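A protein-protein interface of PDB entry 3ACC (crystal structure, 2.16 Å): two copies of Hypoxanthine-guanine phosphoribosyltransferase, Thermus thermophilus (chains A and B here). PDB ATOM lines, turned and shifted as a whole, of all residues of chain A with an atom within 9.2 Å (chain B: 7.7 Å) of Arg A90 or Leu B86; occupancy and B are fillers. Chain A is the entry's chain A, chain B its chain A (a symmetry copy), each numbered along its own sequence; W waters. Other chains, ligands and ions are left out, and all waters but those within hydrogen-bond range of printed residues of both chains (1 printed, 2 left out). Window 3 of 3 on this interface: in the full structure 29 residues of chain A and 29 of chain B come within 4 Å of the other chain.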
ATOM      1  N   HIS A  40     -19.116   6.697 -18.911  1.00  0.00           N
ATOM      2  CA  HIS A  40     -18.495   5.747 -17.997  1.00  0.00           C
ATOM      3  C   HIS A  40     -17.460   6.560 -17.236  1.00  0.00           C
ATOM      4  O   HIS A  40     -16.412   6.907 -17.782  1.00  0.00           O
ATOM      5  CB  HIS A  40     -17.809   4.624 -18.777  1.00  0.00           C
ATOM      6  CG  HIS A  40     -17.035   3.671 -17.918  1.00  0.00           C
ATOM      7  ND1 HIS A  40     -17.627   2.885 -16.951  1.00  0.00           N
ATOM      8  CD2 HIS A  40     -15.715   3.364 -17.895  1.00  0.00           C
ATOM      9  CE1 HIS A  40     -16.707   2.134 -16.372  1.00  0.00           C
ATOM     10  NE2 HIS A  40     -15.537   2.406 -16.927  1.00  0.00           N
ATOM     11  N   ILE A  42     -14.562   7.127 -14.626  1.00  0.00           N
ATOM     12  CA  ILE A  42     -13.482   6.413 -13.953  1.00  0.00           C
ATOM     13  C   ILE A  42     -12.852   7.289 -12.863  1.00  0.00           C
ATOM     14  O   ILE A  42     -12.190   8.282 -13.160  1.00  0.00           O
ATOM     15  CB  ILE A  42     -12.383   6.001 -14.952  1.00  0.00           C
ATOM     16  CG1 ILE A  42     -12.976   5.104 -16.040  1.00  0.00           C
ATOM     17  CG2 ILE A  42     -11.266   5.265 -14.228  1.00  0.00           C
ATOM     18  CD1 ILE A  42     -11.955   4.604 -17.047  1.00  0.00           C
ATOM     19  N   LEU A  45      -8.537   6.781  -7.602  1.00  0.00           N
ATOM     20  CA  LEU A  45      -8.377   6.666  -6.155  1.00  0.00           C
ATOM     21  C   LEU A  45      -6.952   7.051  -5.743  1.00  0.00           C
ATOM     22  O   LEU A  45      -6.028   6.959  -6.552  1.00  0.00           O
ATOM     23  CB  LEU A  45      -8.683   5.227  -5.710  1.00  0.00           C
ATOM     24  CG  LEU A  45     -10.142   4.769  -5.815  1.00  0.00           C
ATOM     25  CD1 LEU A  45     -10.235   3.267  -5.593  1.00  0.00           C
ATOM     26  CD2 LEU A  45     -10.986   5.525  -4.801  1.00  0.00           C
ATOM     27  N   MET A  65     -19.659   3.350 -13.689  1.00  0.00           N
ATOM     28  CA  MET A  65     -18.412   3.844 -13.139  1.00  0.00           C
ATOM     29  C   MET A  65     -17.442   2.750 -12.771  1.00  0.00           C
ATOM     30  O   MET A  65     -17.805   1.581 -12.694  1.00  0.00           O
ATOM     31  CB  MET A  65     -18.679   4.752 -11.927  1.00  0.00           C
ATOM     32  CG  MET A  65     -20.014   4.548 -11.225  1.00  0.00           C
ATOM     33  SD  MET A  65     -20.278   5.731  -9.861  1.00  0.00           S
ATOM     34  CE  MET A  65     -21.797   6.524 -10.350  1.00  0.00           C
ATOM     35  N   ASP A  66     -16.188   3.144 -12.585  1.00  0.00           N
ATOM     36  CA  ASP A  66     -15.143   2.219 -12.190  1.00  0.00           C
ATOM     37  C   ASP A  66     -14.150   2.991 -11.325  1.00  0.00           C
ATOM     38  O   ASP A  66     -14.205   4.218 -11.240  1.00  0.00           O
ATOM     39  CB  ASP A  66     -14.435   1.624 -13.406  1.00  0.00           C
ATOM     40  CG  ASP A  66     -13.925   0.217 -13.144  1.00  0.00           C
ATOM     41  OD1 ASP A  66     -13.804  -0.161 -11.959  1.00  0.00           O
ATOM     42  OD2 ASP A  66     -13.640  -0.508 -14.115  1.00  0.00           O
ATOM     43  N   PHE A  67     -13.249   2.262 -10.682  1.00  0.00           N
ATOM     44  CA  PHE A  67     -12.267   2.864  -9.795  1.00  0.00           C
ATOM     45  C   PHE A  67     -10.896   2.261 -10.055  1.00  0.00           C
ATOM     46  O   PHE A  67     -10.761   1.043 -10.148  1.00  0.00           O
ATOM     47  CB  PHE A  67     -12.667   2.600  -8.342  1.00  0.00           C
ATOM     48  CG  PHE A  67     -13.956   3.257  -7.938  1.00  0.00           C
ATOM     49  CD1 PHE A  67     -13.946   4.430  -7.186  1.00  0.00           C
ATOM     50  CD2 PHE A  67     -15.179   2.724  -8.331  1.00  0.00           C
ATOM     51  CE1 PHE A  67     -15.138   5.064  -6.833  1.00  0.00           C
ATOM     52  CE2 PHE A  67     -16.375   3.348  -7.987  1.00  0.00           C
ATOM     53  CZ  PHE A  67     -16.357   4.522  -7.236  1.00  0.00           C
ATOM     54  N   ILE A  68      -9.882   3.110 -10.185  1.00  0.00           N
ATOM     55  CA  ILE A  68      -8.528   2.621 -10.408  1.00  0.00           C
ATOM     56  C   ILE A  68      -7.515   3.419  -9.591  1.00  0.00           C
ATOM     57  O   ILE A  68      -7.790   4.539  -9.160  1.00  0.00           O
ATOM     58  CB  ILE A  68      -8.130   2.676 -11.908  1.00  0.00           C
ATOM     59  CG1 ILE A  68      -7.773   4.102 -12.330  1.00  0.00           C
ATOM     60  CG2 ILE A  68      -9.261   2.136 -12.753  1.00  0.00           C
ATOM     61  CD1 ILE A  68      -8.883   5.090 -12.191  1.00  0.00           C
ATOM     62  N   LEU A  86      -1.680   0.757  -9.910  1.00  0.00           N
ATOM     63  CA  LEU A  86      -1.918  -0.100  -8.755  1.00  0.00           C
ATOM     64  C   LEU A  86      -3.224  -0.896  -8.828  1.00  0.00           C
ATOM     65  O   LEU A  86      -3.245  -2.086  -8.517  1.00  0.00           O
ATOM     66  CB  LEU A  86      -1.887   0.747  -7.480  1.00  0.00           C
ATOM     67  CG  LEU A  86      -0.603   1.565  -7.300  1.00  0.00           C
ATOM     68  CD1 LEU A  86      -0.702   2.414  -6.045  1.00  0.00           C
ATOM     69  CD2 LEU A  86       0.595   0.631  -7.219  1.00  0.00           C
ATOM     70  N   LYS A  87      -4.309  -0.242  -9.234  1.00  0.00           N
ATOM     71  CA  LYS A  87      -5.604  -0.911  -9.351  1.00  0.00           C
ATOM     72  C   LYS A  87      -6.095  -0.866 -10.799  1.00  0.00           C
ATOM     73  O   LYS A  87      -6.231   0.210 -11.385  1.00  0.00           O
ATOM     74  CB  LYS A  87      -6.633  -0.251  -8.428  1.00  0.00           C
ATOM     75  CG  LYS A  87      -8.009  -0.891  -8.490  1.00  0.00           C
ATOM     76  CD  LYS A  87      -8.982  -0.231  -7.525  1.00  0.00           C
ATOM     77  CE  LYS A  87     -10.390  -0.785  -7.707  1.00  0.00           C
ATOM     78  NZ  LYS A  87     -10.445  -2.262  -7.521  1.00  0.00           N
ATOM     79  N   ASP A  88      -6.367  -2.038 -11.367  1.00  0.00           N
ATOM     80  CA  ASP A  88      -6.814  -2.144 -12.751  1.00  0.00           C
ATOM     81  C   ASP A  88      -8.303  -1.923 -12.989  1.00  0.00           C
ATOM     82  O   ASP A  88      -9.109  -1.922 -12.056  1.00  0.00           O
ATOM     83  CB  ASP A  88      -6.423  -3.508 -13.326  1.00  0.00           C
ATOM     84  CG  ASP A  88      -4.927  -3.673 -13.460  1.00  0.00           C
ATOM     85  OD1 ASP A  88      -4.227  -3.629 -12.427  1.00  0.00           O
ATOM     86  OD2 ASP A  88      -4.452  -3.844 -14.601  1.00  0.00           O
ATOM     87  N   LEU A  89      -8.648  -1.742 -14.261  1.00  0.00           N
ATOM     88  CA  LEU A  89     -10.026  -1.526 -14.684  1.00  0.00           C
ATOM     89  C   LEU A  89     -10.797  -2.834 -14.612  1.00  0.00           C
ATOM     90  O   LEU A  89     -10.237  -3.904 -14.838  1.00  0.00           O
ATOM     91  CB  LEU A  89     -10.063  -1.002 -16.120  1.00  0.00           C
ATOM     92  CG  LEU A  89      -9.520   0.402 -16.388  1.00  0.00           C
ATOM     93  CD1 LEU A  89      -9.527   0.669 -17.884  1.00  0.00           C
ATOM     94  CD2 LEU A  89     -10.370   1.427 -15.661  1.00  0.00           C
ATOM     95  N   ARG A  90     -12.089  -2.742 -14.319  1.00  0.00           N
ATOM     96  CA  ARG A  90     -12.926  -3.926 -14.218  1.00  0.00           C
ATOM     97  C   ARG A  90     -13.969  -3.969 -15.330  1.00  0.00           C
ATOM     98  O   ARG A  90     -14.289  -5.036 -15.847  1.00  0.00           O
ATOM     99  CB  ARG A  90     -13.603  -3.949 -12.850  1.00  0.00           C
ATOM    100  CG  ARG A  90     -14.160  -5.295 -12.443  1.00  0.00           C
ATOM    101  CD  ARG A  90     -14.175  -5.400 -10.933  1.00  0.00           C
ATOM    102  NE  ARG A  90     -12.832  -5.214 -10.388  1.00  0.00           N
ATOM    103  CZ  ARG A  90     -12.555  -5.106  -9.093  1.00  0.00           C
ATOM    104  NH1 ARG A  90     -13.531  -5.166  -8.195  1.00  0.00           N
ATOM    105  NH2 ARG A  90     -11.301  -4.939  -8.693  1.00  0.00           N
ATOM    106  N   LEU A  91     -14.499  -2.806 -15.698  1.00  0.00           N
ATOM    107  CA  LEU A  91     -15.505  -2.727 -16.754  1.00  0.00           C
ATOM    108  C   LEU A  91     -14.854  -2.291 -18.058  1.00  0.00           C
ATOM    109  O   LEU A  91     -13.858  -1.570 -18.051  1.00  0.00           O
ATOM    110  CB  LEU A  91     -16.615  -1.743 -16.375  1.00  0.00           C
ATOM    111  CG  LEU A  91     -17.622  -2.192 -15.310  1.00  0.00           C
ATOM    112  CD1 LEU A  91     -16.914  -2.395 -13.986  1.00  0.00           C
ATOM    113  CD2 LEU A  91     -18.724  -1.150 -15.168  1.00  0.00           C
ATOM    114  N   PRO A  92     -15.402  -2.740 -19.198  1.00  0.00           N
ATOM    115  CA  PRO A  92     -14.864  -2.390 -20.516  1.00  0.00           C
ATOM    116  C   PRO A  92     -14.990  -0.903 -20.818  1.00  0.00           C
ATOM    117  O   PRO A  92     -15.960  -0.265 -20.419  1.00  0.00           O
ATOM    118  CB  PRO A  92     -15.707  -3.237 -21.473  1.00  0.00           C
ATOM    119  CG  PRO A  92     -16.113  -4.413 -20.630  1.00  0.00           C
ATOM    120  CD  PRO A  92     -16.464  -3.755 -19.323  1.00  0.00           C
ATOM    121  N   ILE A  93     -13.998  -0.350 -21.509  1.00  0.00           N
ATOM    122  CA  ILE A  93     -14.041   1.057 -21.883  1.00  0.00           C
ATOM    123  C   ILE A  93     -13.989   1.193 -23.393  1.00  0.00           C
ATOM    124  O   ILE A  93     -14.172   2.286 -23.931  1.00  0.00           O
ATOM    125  CB  ILE A  93     -12.871   1.872 -21.282  1.00  0.00           C
ATOM    126  CG1 ILE A  93     -11.539   1.353 -21.813  1.00  0.00           C
ATOM    127  CG2 ILE A  93     -12.921   1.815 -19.761  1.00  0.00           C
ATOM    128  CD1 ILE A  93     -10.366   2.244 -21.462  1.00  0.00           C
ATOM    129  N   TYR A 117      -2.931   5.152 -21.317  1.00  0.00           N
ATOM    130  CA  TYR A 117      -3.381   3.818 -20.944  1.00  0.00           C
ATOM    131  C   TYR A 117      -4.809   3.580 -21.429  1.00  0.00           C
ATOM    132  O   TYR A 117      -5.104   2.559 -22.056  1.00  0.00           O
ATOM    133  CB  TYR A 117      -3.331   3.656 -19.425  1.00  0.00           C
ATOM    134  CG  TYR A 117      -3.768   2.295 -18.942  1.00  0.00           C
ATOM    135  CD1 TYR A 117      -2.963   1.172 -19.137  1.00  0.00           C
ATOM    136  CD2 TYR A 117      -4.989   2.125 -18.290  1.00  0.00           C
ATOM    137  CE1 TYR A 117      -3.364  -0.085 -18.692  1.00  0.00           C
ATOM    138  CE2 TYR A 117      -5.400   0.873 -17.841  1.00  0.00           C
ATOM    139  CZ  TYR A 117      -4.584  -0.227 -18.046  1.00  0.00           C
ATOM    140  OH  TYR A 117      -4.981  -1.463 -17.597  1.00  0.00           O
ATOM    141  N   LEU A 118      -5.692   4.528 -21.135  1.00  0.00           N
ATOM    142  CA  LEU A 118      -7.089   4.414 -21.532  1.00  0.00           C
ATOM    143  C   LEU A 118      -7.273   4.446 -23.045  1.00  0.00           C
ATOM    144  O   LEU A 118      -8.089   3.703 -23.594  1.00  0.00           O
ATOM    145  CB  LEU A 118      -7.913   5.537 -20.891  1.00  0.00           C
ATOM    146  CG  LEU A 118      -7.996   5.526 -19.359  1.00  0.00           C
ATOM    147  CD1 LEU A 118      -8.810   6.716 -18.877  1.00  0.00           C
ATOM    148  CD2 LEU A 118      -8.628   4.229 -18.890  1.00  0.00           C
ATOM    149  N   ARG A 121      -6.985   1.234 -25.239  1.00  0.00           N
ATOM    150  CA  ARG A 121      -8.151   0.360 -25.338  1.00  0.00           C
ATOM    151  C   ARG A 121      -9.208   0.896 -26.295  1.00  0.00           C
ATOM    152  O   ARG A 121     -10.269   0.294 -26.472  1.00  0.00           O
ATOM    153  CB  ARG A 121      -8.762   0.128 -23.959  1.00  0.00           C
ATOM    154  CG  ARG A 121      -7.820  -0.611 -23.035  1.00  0.00           C
ATOM    155  CD  ARG A 121      -8.570  -1.315 -21.938  1.00  0.00           C
ATOM    156  NE  ARG A 121      -7.659  -2.021 -21.049  1.00  0.00           N
ATOM    157  CZ  ARG A 121      -8.052  -2.881 -20.119  1.00  0.00           C
ATOM    158  NH1 ARG A 121      -9.344  -3.138 -19.963  1.00  0.00           N
ATOM    159  NH2 ARG A 121      -7.155  -3.478 -19.346  1.00  0.00           N
ATOM    160  N   LEU B  45     -15.506  -1.257  -1.774  1.00  0.00           N
ATOM    161  CA  LEU B  45     -15.924  -0.835  -3.107  1.00  0.00           C
ATOM    162  C   LEU B  45     -16.740  -1.941  -3.785  1.00  0.00           C
ATOM    163  O   LEU B  45     -16.596  -3.116  -3.443  1.00  0.00           O
ATOM    164  CB  LEU B  45     -14.691  -0.495  -3.957  1.00  0.00           C
ATOM    165  CG  LEU B  45     -13.904   0.759  -3.559  1.00  0.00           C
ATOM    166  CD1 LEU B  45     -12.586   0.810  -4.316  1.00  0.00           C
ATOM    167  CD2 LEU B  45     -14.743   1.995  -3.839  1.00  0.00           C
ATOM    168  N   ASN B  46     -17.592  -1.583  -4.744  1.00  0.00           N
ATOM    169  CA  ASN B  46     -17.787  -0.204  -5.191  1.00  0.00           C
ATOM    170  C   ASN B  46     -18.991   0.472  -4.536  1.00  0.00           C
ATOM    171  O   ASN B  46     -19.043   1.697  -4.422  1.00  0.00           O
ATOM    172  CB  ASN B  46     -17.999  -0.182  -6.707  1.00  0.00           C
ATOM    173  CG  ASN B  46     -16.755  -0.564  -7.488  1.00  0.00           C
ATOM    174  OD1 ASN B  46     -16.813  -0.759  -8.703  1.00  0.00           O
ATOM    175  ND2 ASN B  46     -15.626  -0.666  -6.800  1.00  0.00           N
ATOM    176  N   ILE B  68     -10.975  -1.357  -0.582  1.00  0.00           N
ATOM    177  CA  ILE B  68     -10.762  -2.723  -1.043  1.00  0.00           C
ATOM    178  C   ILE B  68     -11.998  -3.257  -1.762  1.00  0.00           C
ATOM    179  O   ILE B  68     -13.103  -2.742  -1.591  1.00  0.00           O
ATOM    180  CB  ILE B  68     -10.398  -3.680   0.124  1.00  0.00           C
ATOM    181  CG1 ILE B  68     -11.640  -4.059   0.932  1.00  0.00           C
ATOM    182  CG2 ILE B  68      -9.362  -3.027   1.010  1.00  0.00           C
ATOM    183  CD1 ILE B  68     -12.336  -2.909   1.582  1.00  0.00           C
ATOM    184  N   ALA B  69     -11.797  -4.281  -2.581  1.00  0.00           N
ATOM    185  CA  ALA B  69     -12.884  -4.899  -3.325  1.00  0.00           C
ATOM    186  C   ALA B  69     -12.942  -6.376  -2.948  1.00  0.00           C
ATOM    187  O   ALA B  69     -11.904  -7.018  -2.779  1.00  0.00           O
ATOM    188  CB  ALA B  69     -12.644  -4.742  -4.817  1.00  0.00           C
ATOM    189  N   ILE B  70     -14.150  -6.912  -2.806  1.00  0.00           N
ATOM    190  CA  ILE B  70     -14.319  -8.315  -2.441  1.00  0.00           C
ATOM    191  C   ILE B  70     -15.619  -8.891  -3.006  1.00  0.00           C
ATOM    192  O   ILE B  70     -16.615  -8.182  -3.144  1.00  0.00           O
ATOM    193  CB  ILE B  70     -14.307  -8.493  -0.902  1.00  0.00           C
ATOM    194  CG1 ILE B  70     -14.420  -9.977  -0.546  1.00  0.00           C
ATOM    195  CG2 ILE B  70     -15.447  -7.700  -0.275  1.00  0.00           C
ATOM    196  CD1 ILE B  70     -14.360 -10.258   0.940  1.00  0.00           C
ATOM    197  N   SER B  71     -15.597 -10.180  -3.332  1.00  0.00           N
ATOM    198  CA  SER B  71     -16.769 -10.854  -3.881  1.00  0.00           C
ATOM    199  C   SER B  71     -17.133 -12.098  -3.075  1.00  0.00           C
ATOM    200  O   SER B  71     -16.271 -12.721  -2.456  1.00  0.00           O
ATOM    201  CB  SER B  71     -16.516 -11.239  -5.339  1.00  0.00           C
ATOM    202  OG  SER B  71     -16.259 -10.090  -6.126  1.00  0.00           O
ATOM    203  N   SER B  72     -18.414 -12.456  -3.094  1.00  0.00           N
ATOM    204  CA  SER B  72     -18.902 -13.619  -2.359  1.00  0.00           C
ATOM    205  C   SER B  72     -18.180 -14.904  -2.757  1.00  0.00           C
ATOM    206  O   SER B  72     -17.973 -15.174  -3.940  1.00  0.00           O
ATOM    207  CB  SER B  72     -20.408 -13.783  -2.579  1.00  0.00           C
ATOM    208  OG  SER B  72     -20.935 -14.816  -1.764  1.00  0.00           O
ATOM    209  N   LEU B  85     -11.536 -11.470  -2.878  1.00  0.00           N
ATOM    210  CA  LEU B  85     -10.655 -10.350  -2.562  1.00  0.00           C
ATOM    211  C   LEU B  85     -10.036  -9.785  -3.837  1.00  0.00           C
ATOM    212  O   LEU B  85      -8.902 -10.110  -4.189  1.00  0.00           O
ATOM    213  CB  LEU B  85      -9.551 -10.805  -1.603  1.00  0.00           C
ATOM    214  CG  LEU B  85      -8.586  -9.723  -1.114  1.00  0.00           C
ATOM    215  CD1 LEU B  85      -9.357  -8.612  -0.423  1.00  0.00           C
ATOM    216  CD2 LEU B  85      -7.570 -10.342  -0.167  1.00  0.00           C
ATOM    217  N   LEU B  86     -10.791  -8.930  -4.520  1.00  0.00           N
ATOM    218  CA  LEU B  86     -10.344  -8.321  -5.767  1.00  0.00           C
ATOM    219  C   LEU B  86      -9.294  -7.222  -5.582  1.00  0.00           C
ATOM    220  O   LEU B  86      -8.307  -7.175  -6.315  1.00  0.00           O
ATOM    221  CB  LEU B  86     -11.554  -7.772  -6.527  1.00  0.00           C
ATOM    222  CG  LEU B  86     -12.656  -8.806  -6.786  1.00  0.00           C
ATOM    223  CD1 LEU B  86     -13.831  -8.146  -7.483  1.00  0.00           C
ATOM    224  CD2 LEU B  86     -12.103  -9.945  -7.632  1.00  0.00           C
ATOM    225  N   LYS B  87      -9.506  -6.341  -4.609  1.00  0.00           N
ATOM    226  CA  LYS B  87      -8.560  -5.258  -4.338  1.00  0.00           C
ATOM    227  C   LYS B  87      -8.001  -5.384  -2.920  1.00  0.00           C
ATOM    228  O   LYS B  87      -8.756  -5.406  -1.946  1.00  0.00           O
ATOM    229  CB  LYS B  87      -9.240  -3.896  -4.517  1.00  0.00           C
ATOM    230  CG  LYS B  87      -8.320  -2.716  -4.255  1.00  0.00           C
ATOM    231  CD  LYS B  87      -9.026  -1.389  -4.487  1.00  0.00           C
ATOM    232  CE  LYS B  87      -8.137  -0.220  -4.078  1.00  0.00           C
ATOM    233  NZ  LYS B  87      -6.837  -0.216  -4.807  1.00  0.00           N
ATOM    234  N   ASP B  88      -6.677  -5.456  -2.813  1.00  0.00           N
ATOM    235  CA  ASP B  88      -6.012  -5.609  -1.524  1.00  0.00           C
ATOM    236  C   ASP B  88      -5.794  -4.327  -0.731  1.00  0.00           C
ATOM    237  O   ASP B  88      -5.925  -3.218  -1.254  1.00  0.00           O
ATOM    238  CB  ASP B  88      -4.662  -6.306  -1.709  1.00  0.00           C
ATOM    239  CG  ASP B  88      -4.808  -7.740  -2.165  1.00  0.00           C
ATOM    240  OD1 ASP B  88      -5.355  -7.963  -3.264  1.00  0.00           O
ATOM    241  OD2 ASP B  88      -4.375  -8.643  -1.421  1.00  0.00           O
ATOM    242  N   GLN B 165     -24.740  -2.351 -12.741  1.00  0.00           N
ATOM    243  CA  GLN B 165     -23.739  -1.301 -12.935  1.00  0.00           C
ATOM    244  C   GLN B 165     -24.286   0.122 -13.117  1.00  0.00           C
ATOM    245  O   GLN B 165     -23.529   1.094 -13.060  1.00  0.00           O
ATOM    246  CB  GLN B 165     -22.821  -1.652 -14.113  1.00  0.00           C
ATOM    247  CG  GLN B 165     -21.946  -2.882 -13.879  1.00  0.00           C
ATOM    248  CD  GLN B 165     -21.155  -2.813 -12.574  1.00  0.00           C
ATOM    249  OE1 GLN B 165     -20.703  -1.741 -12.159  1.00  0.00           O
ATOM    250  NE2 GLN B 165     -20.976  -3.960 -11.930  1.00  0.00           N
HETATM  251  O   HOH W   1     -21.110   1.102 -12.183  1.00  0.00           O
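The backbone NH of Lys B87 is in hydrogen-bond range of the backbone carbonyl oxygen of Ala B69 (3.1 Å).
N of Leu B86 sits at hydrogen-bond distance from O of Ala B69 (2.8 Å).
The backbone carbonyl oxygen (O) of Ile B68 lies within hydrogen-bond range of the backbone NH (N) of Leu B45 (2.8 Å).
N of Arg A90 sits at hydrogen-bond distance from OD2 of Asp A66, at 2.7 Å.
OD2 of Asp A66 sits at hydrogen-bond distance from N of Leu A91 (2.9 Å).
N of Leu A45 lies within hydrogen-bond range of O of Ile A68.
Among the printed residues, merely in contact across the chains: Leu A45 with Leu B45 (3.6 Å), Phe A67 with Asn B46 (3.7 Å), Lys A87 with Lys B87 (3.3 Å), Arg A90 with Ala B69 (3.5 Å), Arg A90 with Leu B86 (3.1 Å) and Leu A91 with Gln B165 (3.6 Å).
Of the 18 printed residues of chain A, 5 touch a printed residue of chain B.
Printed residues of chain A that touch a printed residue of chain B: Leu A45, Phe A67, Lys A87, Arg A90 and Leu A91.
Hydrophobic or aromatic side chains of chain A within 4 Å of the printed part of chain B: Leu A45, Phe A67 and Leu A91.
Among the printed residues, 6 pairs touch across the chains.
Leu A45 touches its own counterpart, Leu B45.
Lys A87 touches its own counterpart, Lys B87.
Of the 6 pairs that touch across the chains among the printed residues, 2 have their exchanged pair printed and touching as well.
Arg A90 touches just these residues of chain B: Ala B69 (3.5 Å) and Leu B86 (3.1 Å).
Of the printed residues of chain A, Leu B86 touches Arg A90.
Of chain A, only Arg A90 comes within 4 Å of Ala B69.
Of the printed residues of chain B, Leu A91 touches Gln B165 (3.6 Å).
Of the printed residues of chain A, Leu B45 touches Leu A45 (3.6 Å).
Pro A92 touches none of the printed residues of chain B.
Ile A68 touches none of the printed residues of chain B.
The nearest residue of chain A that does not touch Leu B86 is Lys A87 (5.4 Å).
The nearest printed residue of chain B that does not touch Phe A67 is Leu B45 (4.2 Å).
Water W1 lies within hydrogen-bond range of the backbone carbonyl oxygen (O) of Gln B165 (2.6 Å) and the backbone NH (N) of Met A65 (3.1 Å).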
